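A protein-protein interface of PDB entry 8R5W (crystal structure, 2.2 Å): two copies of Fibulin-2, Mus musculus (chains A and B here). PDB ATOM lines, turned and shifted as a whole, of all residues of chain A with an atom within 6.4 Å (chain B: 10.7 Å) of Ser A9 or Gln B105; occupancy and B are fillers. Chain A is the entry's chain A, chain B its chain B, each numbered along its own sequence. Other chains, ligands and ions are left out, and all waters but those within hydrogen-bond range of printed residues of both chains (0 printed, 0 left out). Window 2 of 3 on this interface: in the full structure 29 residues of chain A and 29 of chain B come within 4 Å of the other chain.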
ATOM      1  N   HIS A   7     -10.127  24.100  16.727  1.00  0.00           N
ATOM      2  CA  HIS A   7     -11.292  24.812  17.224  1.00  0.00           C
ATOM      3  C   HIS A   7     -11.687  25.852  16.182  1.00  0.00           C
ATOM      4  O   HIS A   7     -11.479  27.056  16.343  1.00  0.00           O
ATOM      5  CB  HIS A   7     -10.994  25.407  18.604  1.00  0.00           C
ATOM      6  CG  HIS A   7     -10.481  24.413  19.585  1.00  0.00           C
ATOM      7  ND1 HIS A   7     -11.318  23.416  20.021  1.00  0.00           N
ATOM      8  CD2 HIS A   7      -9.294  24.205  20.176  1.00  0.00           C
ATOM      9  CE1 HIS A   7     -10.674  22.659  20.891  1.00  0.00           C
ATOM     10  NE2 HIS A   7      -9.438  23.117  20.987  1.00  0.00           N
ATOM     11  N   MET A   8     -12.202  25.348  15.069  1.00  0.00           N
ATOM     12  CA  MET A   8     -12.685  26.206  14.001  1.00  0.00           C
ATOM     13  C   MET A   8     -14.196  26.339  14.181  1.00  0.00           C
ATOM     14  O   MET A   8     -14.873  25.356  14.457  1.00  0.00           O
ATOM     15  CB  MET A   8     -12.258  25.605  12.649  1.00  0.00           C
ATOM     16  CG  MET A   8     -12.687  26.389  11.436  1.00  0.00           C
ATOM     17  SD  MET A   8     -11.744  26.048   9.939  1.00  0.00           S
ATOM     18  CE  MET A   8     -10.159  26.759  10.403  1.00  0.00           C
ATOM     19  N   SER A   9     -14.726  27.553  14.023  1.00  0.00           N
ATOM     20  CA  SER A   9     -16.173  27.759  14.003  1.00  0.00           C
ATOM     21  C   SER A   9     -16.841  26.890  12.932  1.00  0.00           C
ATOM     22  O   SER A   9     -16.188  26.420  11.981  1.00  0.00           O
ATOM     23  CB  SER A   9     -16.528  29.201  13.829  1.00  0.00           C
ATOM     24  OG  SER A   9     -16.307  29.607  12.492  1.00  0.00           O
ATOM     25  N   THR A  10     -18.155  26.676  13.106  1.00  0.00           N
ATOM     26  CA  THR A  10     -18.940  25.916  12.151  1.00  0.00           C
ATOM     27  C   THR A  10     -19.001  26.655  10.816  1.00  0.00           C
ATOM     28  O   THR A  10     -18.918  26.026   9.763  1.00  0.00           O
ATOM     29  CB  THR A  10     -20.327  25.661  12.714  1.00  0.00           C
ATOM     30  OG1 THR A  10     -20.128  24.908  13.901  1.00  0.00           O
ATOM     31  CG2 THR A  10     -21.178  24.805  11.802  1.00  0.00           C
ATOM     32  N   LYS A  11     -19.129  27.988  10.877  1.00  0.00           N
ATOM     33  CA  LYS A  11     -19.219  28.802   9.675  1.00  0.00           C
ATOM     34  C   LYS A  11     -17.944  28.653   8.846  1.00  0.00           C
ATOM     35  O   LYS A  11     -18.008  28.454   7.635  1.00  0.00           O
ATOM     36  CB  LYS A  11     -19.501  30.253  10.064  1.00  0.00           C
ATOM     37  CG  LYS A  11     -19.291  31.290   8.987  1.00  0.00           C
ATOM     38  CD  LYS A  11     -20.138  32.540   9.180  1.00  0.00           C
ATOM     39  CE  LYS A  11     -20.102  33.137  10.555  1.00  0.00           C
ATOM     40  NZ  LYS A  11     -21.049  34.249  10.558  1.00  0.00           N
ATOM     41  N   ASP A  12     -16.785  28.754   9.504  1.00  0.00           N
ATOM     42  CA  ASP A  12     -15.510  28.694   8.814  1.00  0.00           C
ATOM     43  C   ASP A  12     -15.279  27.295   8.259  1.00  0.00           C
ATOM     44  O   ASP A  12     -14.676  27.131   7.198  1.00  0.00           O
ATOM     45  CB  ASP A  12     -14.369  29.151   9.707  1.00  0.00           C
ATOM     46  CG  ASP A  12     -14.327  30.649   9.976  1.00  0.00           C
ATOM     47  OD1 ASP A  12     -15.256  31.349   9.530  1.00  0.00           O
ATOM     48  OD2 ASP A  12     -13.364  31.094  10.637  1.00  0.00           O
ATOM     49  N   LEU A  13     -15.726  26.290   9.007  1.00  0.00           N
ATOM     50  CA  LEU A  13     -15.500  24.930   8.597  1.00  0.00           C
ATOM     51  C   LEU A  13     -16.302  24.626   7.335  1.00  0.00           C
ATOM     52  O   LEU A  13     -15.802  23.938   6.439  1.00  0.00           O
ATOM     53  CB  LEU A  13     -15.903  24.046   9.770  1.00  0.00           C
ATOM     54  CG  LEU A  13     -15.553  22.579   9.651  1.00  0.00           C
ATOM     55  CD1 LEU A  13     -14.093  22.321   9.356  1.00  0.00           C
ATOM     56  CD2 LEU A  13     -15.890  22.017  11.068  1.00  0.00           C
ATOM     57  N   ILE A  14     -17.512  25.199   7.265  1.00  0.00           N
ATOM     58  CA  ILE A  14     -18.381  25.061   6.113  1.00  0.00           C
ATOM     59  C   ILE A  14     -17.699  25.664   4.894  1.00  0.00           C
ATOM     60  O   ILE A  14     -17.617  24.995   3.859  1.00  0.00           O
ATOM     61  CB  ILE A  14     -19.783  25.653   6.343  1.00  0.00           C
ATOM     62  CG1 ILE A  14     -20.602  24.813   7.282  1.00  0.00           C
ATOM     63  CG2 ILE A  14     -20.544  25.840   5.017  1.00  0.00           C
ATOM     64  CD1 ILE A  14     -21.777  25.569   7.895  1.00  0.00           C
ATOM     65  N   ILE A  43     -20.155  18.095   9.684  1.00  0.00           N
ATOM     66  CA  ILE A  43     -20.255  19.430   9.114  1.00  0.00           C
ATOM     67  C   ILE A  43     -19.374  19.521   7.865  1.00  0.00           C
ATOM     68  O   ILE A  43     -19.821  19.996   6.813  1.00  0.00           O
ATOM     69  CB  ILE A  43     -19.832  20.508  10.126  1.00  0.00           C
ATOM     70  CG1 ILE A  43     -20.698  20.502  11.393  1.00  0.00           C
ATOM     71  CG2 ILE A  43     -19.734  21.891   9.451  1.00  0.00           C
ATOM     72  CD1 ILE A  43     -22.143  20.855  11.127  1.00  0.00           C
ATOM     73  N   LEU B  96     -26.588  22.409   9.256  1.00  0.00           N
ATOM     74  CA  LEU B  96     -25.503  23.372   9.137  1.00  0.00           C
ATOM     75  C   LEU B  96     -25.936  24.719   9.701  1.00  0.00           C
ATOM     76  O   LEU B  96     -25.198  25.321  10.468  1.00  0.00           O
ATOM     77  CB  LEU B  96     -25.018  23.547   7.703  1.00  0.00           C
ATOM     78  CG  LEU B  96     -24.338  22.337   7.051  1.00  0.00           C
ATOM     79  CD1 LEU B  96     -23.968  22.625   5.610  1.00  0.00           C
ATOM     80  CD2 LEU B  96     -23.141  21.889   7.853  1.00  0.00           C
ATOM     81  N   GLY B  97     -27.093  25.204   9.242  1.00  0.00           N
ATOM     82  CA  GLY B  97     -27.619  26.499   9.638  1.00  0.00           C
ATOM     83  C   GLY B  97     -27.909  26.546  11.134  1.00  0.00           C
ATOM     84  O   GLY B  97     -27.633  27.548  11.785  1.00  0.00           O
ATOM     85  N   LEU B  98     -28.465  25.451  11.669  1.00  0.00           N
ATOM     86  CA  LEU B  98     -28.798  25.381  13.078  1.00  0.00           C
ATOM     87  C   LEU B  98     -27.544  25.509  13.922  1.00  0.00           C
ATOM     88  O   LEU B  98     -27.557  26.198  14.936  1.00  0.00           O
ATOM     89  CB  LEU B  98     -29.548  24.088  13.390  1.00  0.00           C
ATOM     90  CG  LEU B  98     -30.978  23.990  12.829  1.00  0.00           C
ATOM     91  CD1 LEU B  98     -31.613  22.659  13.209  1.00  0.00           C
ATOM     92  CD2 LEU B  98     -31.875  25.140  13.339  1.00  0.00           C
ATOM     93  N   ARG B  99     -26.469  24.826  13.507  1.00  0.00           N
ATOM     94  CA  ARG B  99     -25.248  24.760  14.301  1.00  0.00           C
ATOM     95  C   ARG B  99     -24.577  26.133  14.318  1.00  0.00           C
ATOM     96  O   ARG B  99     -24.053  26.531  15.345  1.00  0.00           O
ATOM     97  CB  ARG B  99     -24.294  23.674  13.798  1.00  0.00           C
ATOM     98  CG  ARG B  99     -23.568  22.901  14.897  1.00  0.00           C
ATOM     99  CD  ARG B  99     -24.502  21.863  15.552  1.00  0.00           C
ATOM    100  NE  ARG B  99     -24.813  20.747  14.642  1.00  0.00           N
ATOM    101  CZ  ARG B  99     -23.924  19.847  14.201  1.00  0.00           C
ATOM    102  NH1 ARG B  99     -22.703  19.793  14.728  1.00  0.00           N
ATOM    103  NH2 ARG B  99     -24.272  19.022  13.222  1.00  0.00           N
ATOM    104  N   VAL B 100     -24.629  26.854  13.189  1.00  0.00           N
ATOM    105  CA  VAL B 100     -24.080  28.199  13.085  1.00  0.00           C
ATOM    106  C   VAL B 100     -24.872  29.137  14.004  1.00  0.00           C
ATOM    107  O   VAL B 100     -24.292  29.945  14.721  1.00  0.00           O
ATOM    108  CB  VAL B 100     -24.089  28.744  11.641  1.00  0.00           C
ATOM    109  CG1 VAL B 100     -23.732  30.232  11.593  1.00  0.00           C
ATOM    110  CG2 VAL B 100     -23.175  27.946  10.715  1.00  0.00           C
ATOM    111  N   ARG B 101     -26.205  29.038  13.946  1.00  0.00           N
ATOM    112  CA  ARG B 101     -27.071  29.864  14.759  1.00  0.00           C
ATOM    113  C   ARG B 101     -26.829  29.573  16.241  1.00  0.00           C
ATOM    114  O   ARG B 101     -26.768  30.492  17.048  1.00  0.00           O
ATOM    115  CB  ARG B 101     -28.535  29.569  14.424  1.00  0.00           C
ATOM    116  CG  ARG B 101     -29.541  30.473  15.126  1.00  0.00           C
ATOM    117  CD  ARG B 101     -30.806  29.700  15.516  1.00  0.00           C
ATOM    118  NE  ARG B 101     -32.033  30.392  15.104  1.00  0.00           N
ATOM    119  CZ  ARG B 101     -33.214  29.789  14.986  1.00  0.00           C
ATOM    120  NH1 ARG B 101     -33.334  28.497  15.245  1.00  0.00           N
ATOM    121  NH2 ARG B 101     -34.281  30.483  14.629  1.00  0.00           N
ATOM    122  N   ALA B 102     -26.650  28.293  16.578  1.00  0.00           N
ATOM    123  CA  ALA B 102     -26.417  27.863  17.952  1.00  0.00           C
ATOM    124  C   ALA B 102     -25.118  28.448  18.503  1.00  0.00           C
ATOM    125  O   ALA B 102     -24.991  28.611  19.705  1.00  0.00           O
ATOM    126  CB  ALA B 102     -26.419  26.344  18.031  1.00  0.00           C
ATOM    127  N   GLU B 103     -24.166  28.773  17.629  1.00  0.00           N
ATOM    128  CA  GLU B 103     -22.899  29.365  18.038  1.00  0.00           C
ATOM    129  C   GLU B 103     -23.005  30.884  18.171  1.00  0.00           C
ATOM    130  O   GLU B 103     -22.017  31.541  18.485  1.00  0.00           O
ATOM    131  CB  GLU B 103     -21.788  29.031  17.046  1.00  0.00           C
ATOM    132  CG  GLU B 103     -21.287  27.603  17.132  1.00  0.00           C
ATOM    133  CD  GLU B 103     -20.330  27.281  15.974  1.00  0.00           C
ATOM    134  OE1 GLU B 103     -20.469  27.881  14.878  1.00  0.00           O
ATOM    135  OE2 GLU B 103     -19.402  26.446  16.128  1.00  0.00           O
ATOM    136  N   GLY B 104     -24.195  31.446  17.932  1.00  0.00           N
ATOM    137  CA  GLY B 104     -24.410  32.879  18.072  1.00  0.00           C
ATOM    138  C   GLY B 104     -23.905  33.656  16.854  1.00  0.00           C
ATOM    139  O   GLY B 104     -23.814  34.880  16.908  1.00  0.00           O
ATOM    140  N   GLN B 105     -23.580  32.959  15.754  1.00  0.00           N
ATOM    141  CA  GLN B 105     -22.990  33.604  14.597  1.00  0.00           C
ATOM    142  C   GLN B 105     -24.059  33.872  13.542  1.00  0.00           C
ATOM    143  O   GLN B 105     -25.089  33.217  13.505  1.00  0.00           O
ATOM    144  CB  GLN B 105     -21.861  32.745  14.025  1.00  0.00           C
ATOM    145  CG  GLN B 105     -20.614  32.707  14.905  1.00  0.00           C
ATOM    146  CD  GLN B 105     -19.425  32.075  14.198  1.00  0.00           C
ATOM    147  OE1 GLN B 105     -19.559  31.047  13.516  1.00  0.00           O
ATOM    148  NE2 GLN B 105     -18.252  32.685  14.322  1.00  0.00           N
ATOM    149  N   SER B 106     -23.765  34.859  12.694  1.00  0.00           N
ATOM    150  CA  SER B 106     -24.640  35.270  11.615  1.00  0.00           C
ATOM    151  C   SER B 106     -24.439  34.357  10.409  1.00  0.00           C
ATOM    152  O   SER B 106     -23.374  33.802  10.178  1.00  0.00           O
ATOM    153  CB  SER B 106     -24.373  36.709  11.244  1.00  0.00           C
ATOM    154  OG  SER B 106     -23.056  36.877  10.719  1.00  0.00           O
ATOM    155  N   CYS B 107     -25.502  34.203   9.641  1.00  0.00           N
ATOM    156  CA  CYS B 107     -25.523  33.295   8.515  1.00  0.00           C
ATOM    157  C   CYS B 107     -24.944  33.971   7.282  1.00  0.00           C
ATOM    158  O   CYS B 107     -25.190  35.165   7.077  1.00  0.00           O
ATOM    159  CB  CYS B 107     -26.977  32.885   8.298  1.00  0.00           C
ATOM    160  SG  CYS B 107     -27.902  32.802   9.853  1.00  0.00           S
ATOM    161  N   GLU B 108     -24.156  33.224   6.498  1.00  0.00           N
ATOM    162  CA  GLU B 108     -23.636  33.740   5.241  1.00  0.00           C
ATOM    163  C   GLU B 108     -24.082  32.831   4.100  1.00  0.00           C
ATOM    164  O   GLU B 108     -23.895  31.631   4.159  1.00  0.00           O
ATOM    165  CB  GLU B 108     -22.122  33.944   5.327  1.00  0.00           C
ATOM    166  CG  GLU B 108     -21.679  35.399   5.467  1.00  0.00           C
ATOM    167  CD  GLU B 108     -20.175  35.596   5.527  1.00  0.00           C
ATOM    168  OE1 GLU B 108     -19.473  35.077   4.628  1.00  0.00           O
ATOM    169  OE2 GLU B 108     -19.713  36.276   6.468  1.00  0.00           O
ATOM    170  N   SER B 109     -24.706  33.421   3.082  1.00  0.00           N
ATOM    171  CA  SER B 109     -25.074  32.715   1.865  1.00  0.00           C
ATOM    172  C   SER B 109     -23.831  32.081   1.248  1.00  0.00           C
ATOM    173  O   SER B 109     -22.810  32.748   1.117  1.00  0.00           O
ATOM    174  CB  SER B 109     -25.748  33.645   0.903  1.00  0.00           C
ATOM    175  OG  SER B 109     -26.015  32.982  -0.319  1.00  0.00           O
ATOM    176  N   MET B 121     -30.094  25.965   4.393  1.00  0.00           N
ATOM    177  CA  MET B 121     -29.180  26.324   5.455  1.00  0.00           C
ATOM    178  C   MET B 121     -29.514  27.713   6.001  1.00  0.00           C
ATOM    179  O   MET B 121     -29.568  27.892   7.212  1.00  0.00           O
ATOM    180  CB  MET B 121     -27.726  26.262   4.987  1.00  0.00           C
ATOM    181  CG  MET B 121     -26.747  26.644   6.086  1.00  0.00           C
ATOM    182  SD  MET B 121     -25.112  26.925   5.421  1.00  0.00           S
ATOM    183  CE  MET B 121     -25.362  28.489   4.576  1.00  0.00           C
ATOM    184  N   LEU B 122     -29.721  28.687   5.110  1.00  0.00           N
ATOM    185  CA  LEU B 122     -29.998  30.057   5.518  1.00  0.00           C
ATOM    186  C   LEU B 122     -31.287  30.120   6.317  1.00  0.00           C
ATOM    187  O   LEU B 122     -31.333  30.756   7.359  1.00  0.00           O
ATOM    188  CB  LEU B 122     -30.086  30.989   4.305  1.00  0.00           C
ATOM    189  CG  LEU B 122     -28.757  31.348   3.649  1.00  0.00           C
ATOM    190  CD1 LEU B 122     -28.986  32.014   2.316  1.00  0.00           C
ATOM    191  CD2 LEU B 122     -27.935  32.242   4.572  1.00  0.00           C
ATOM    192  N   CYS B 124     -32.804  27.859   8.039  1.00  0.00           N
ATOM    193  CA  CYS B 124     -32.654  27.265   9.361  1.00  0.00           C
ATOM    194  C   CYS B 124     -31.740  28.088  10.259  1.00  0.00           C
ATOM    195  O   CYS B 124     -31.836  28.001  11.480  1.00  0.00           O
ATOM    196  CB  CYS B 124     -32.079  25.863   9.283  1.00  0.00           C
ATOM    197  SG  CYS B 124     -33.313  24.739   8.611  1.00  0.00           S
ATOM    198  N   CYS B 125     -30.850  28.877   9.650  1.00  0.00           N
ATOM    199  CA  CYS B 125     -29.930  29.698  10.403  1.00  0.00           C
ATOM    200  C   CYS B 125     -30.617  30.964  10.937  1.00  0.00           C
ATOM    201  O   CYS B 125     -30.248  31.463  11.991  1.00  0.00           O
ATOM    202  CB  CYS B 125     -28.727  30.033   9.535  1.00  0.00           C
ATOM    203  SG  CYS B 125     -27.430  30.894  10.448  1.00  0.00           S
ATOM    204  N   GLU B 126     -31.585  31.497  10.196  1.00  0.00           N
ATOM    205  CA  GLU B 126     -32.142  32.817  10.479  1.00  0.00           C
ATOM    206  C   GLU B 126     -33.377  32.682  11.359  1.00  0.00           C
ATOM    207  O   GLU B 126     -34.072  31.684  11.276  1.00  0.00           O
ATOM    208  CB  GLU B 126     -32.433  33.602   9.200  1.00  0.00           C
ATOM    209  CG  GLU B 126     -33.513  32.988   8.309  1.00  0.00           C
ATOM    210  CD  GLU B 126     -33.374  33.282   6.824  1.00  0.00           C
ATOM    211  OE1 GLU B 126     -32.296  33.755   6.403  1.00  0.00           O
ATOM    212  OE2 GLU B 126     -34.351  33.015   6.089  1.00  0.00           O
ATOM    213  N   GLY B 127     -33.633  33.682  12.203  1.00  0.00           N
ATOM    214  CA  GLY B 127     -34.729  33.602  13.160  1.00  0.00           C
ATOM    215  C   GLY B 127     -35.046  34.955  13.770  1.00  0.00           C
ATOM    216  O   GLY B 127     -35.548  35.807  13.010  1.00  0.00           O
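OG1 of Thr A10 sits at hydrogen-bond distance from OE2 of Glu B103 (2.8 Å). The side-chain hydroxyl of Ser B106 is in hydrogen-bond range of the side-chain amino group of Lys A11, at 3.3 Å.
OG of Ser A9 sits at hydrogen-bond distance from N of Asp A12, 3.1 Å away. The backbone carbonyl oxygen (O) of Val B100 lies within hydrogen-bond range of the backbone NH (N) of Gln B105, at 3.3 Å. The side-chain sulfur of Cys B107 forms a disulfide with the side-chain sulfur of Cys B125, at 2.1 Å.
Among the printed residues, merely in contact across the chains: Ser A9 with Gln B105 (3.6 Å), Thr A10 with Arg B99 (3.9 Å), Thr A10 with Val B100 (3.9 Å), Lys A11 with Gln B105 (3.5 Å), Ile A14 with Leu B96 (3.8 Å), Ile A14 with Val B100 (3.9 Å), Ile A43 with Leu B96 (3.6 Å) and Ile A43 with Arg B99 (3.5 Å).
Of chain B, only Gln B105 comes within 4 Å of Ser A9. Of chain B, only Arg B99 (3.9 Å), Val B100 (3.9 Å) and Glu B103 (2.8 Å) come within 4 Å of Thr A10. No residue of chain B comes within 4 Å of Asp A12. Of the printed residues of chain B, Ile A43 touches Leu B96 and Arg B99. Printed residues of chain A within 4 Å of Leu B96: Ile A14 (3.8 Å) and Ile A43 (3.6 Å). Leu B98 touches none of the printed residues of chain A. Of the printed residues of chain A, Arg B99 touches Thr A10 and Ile A43. Printed residues of chain A within 4 Å of Val B100: Thr A10 (3.9 Å) and Ile A14 (3.9 Å). Of the printed residues of chain A, Glu B103 touches Thr A10 (2.8 Å). Gln B105 touches just these residues of chain A: Ser A9 (3.6 Å) and Lys A11 (3.5 Å). Glu B126 touches none of the printed residues of chain A. The nearest residue of chain A that does not touch Gln B105 is Thr A10 (4.6 Å).
Hydrophobic or aromatic side chains of chain A that line the printed part of chain B: Ile A14 and Ile A43. Among the printed residues, 10 pairs touch across the chains. Among the printed residues, no Asp or Glu carboxylate lies within 4 Å of a Lys or Arg side-chain nitrogen of the other chain.
No position is printed for both chains. Of the 10 pairs that touch across the chains among the printed residues, none has its exchanged pair printed and touching as well.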
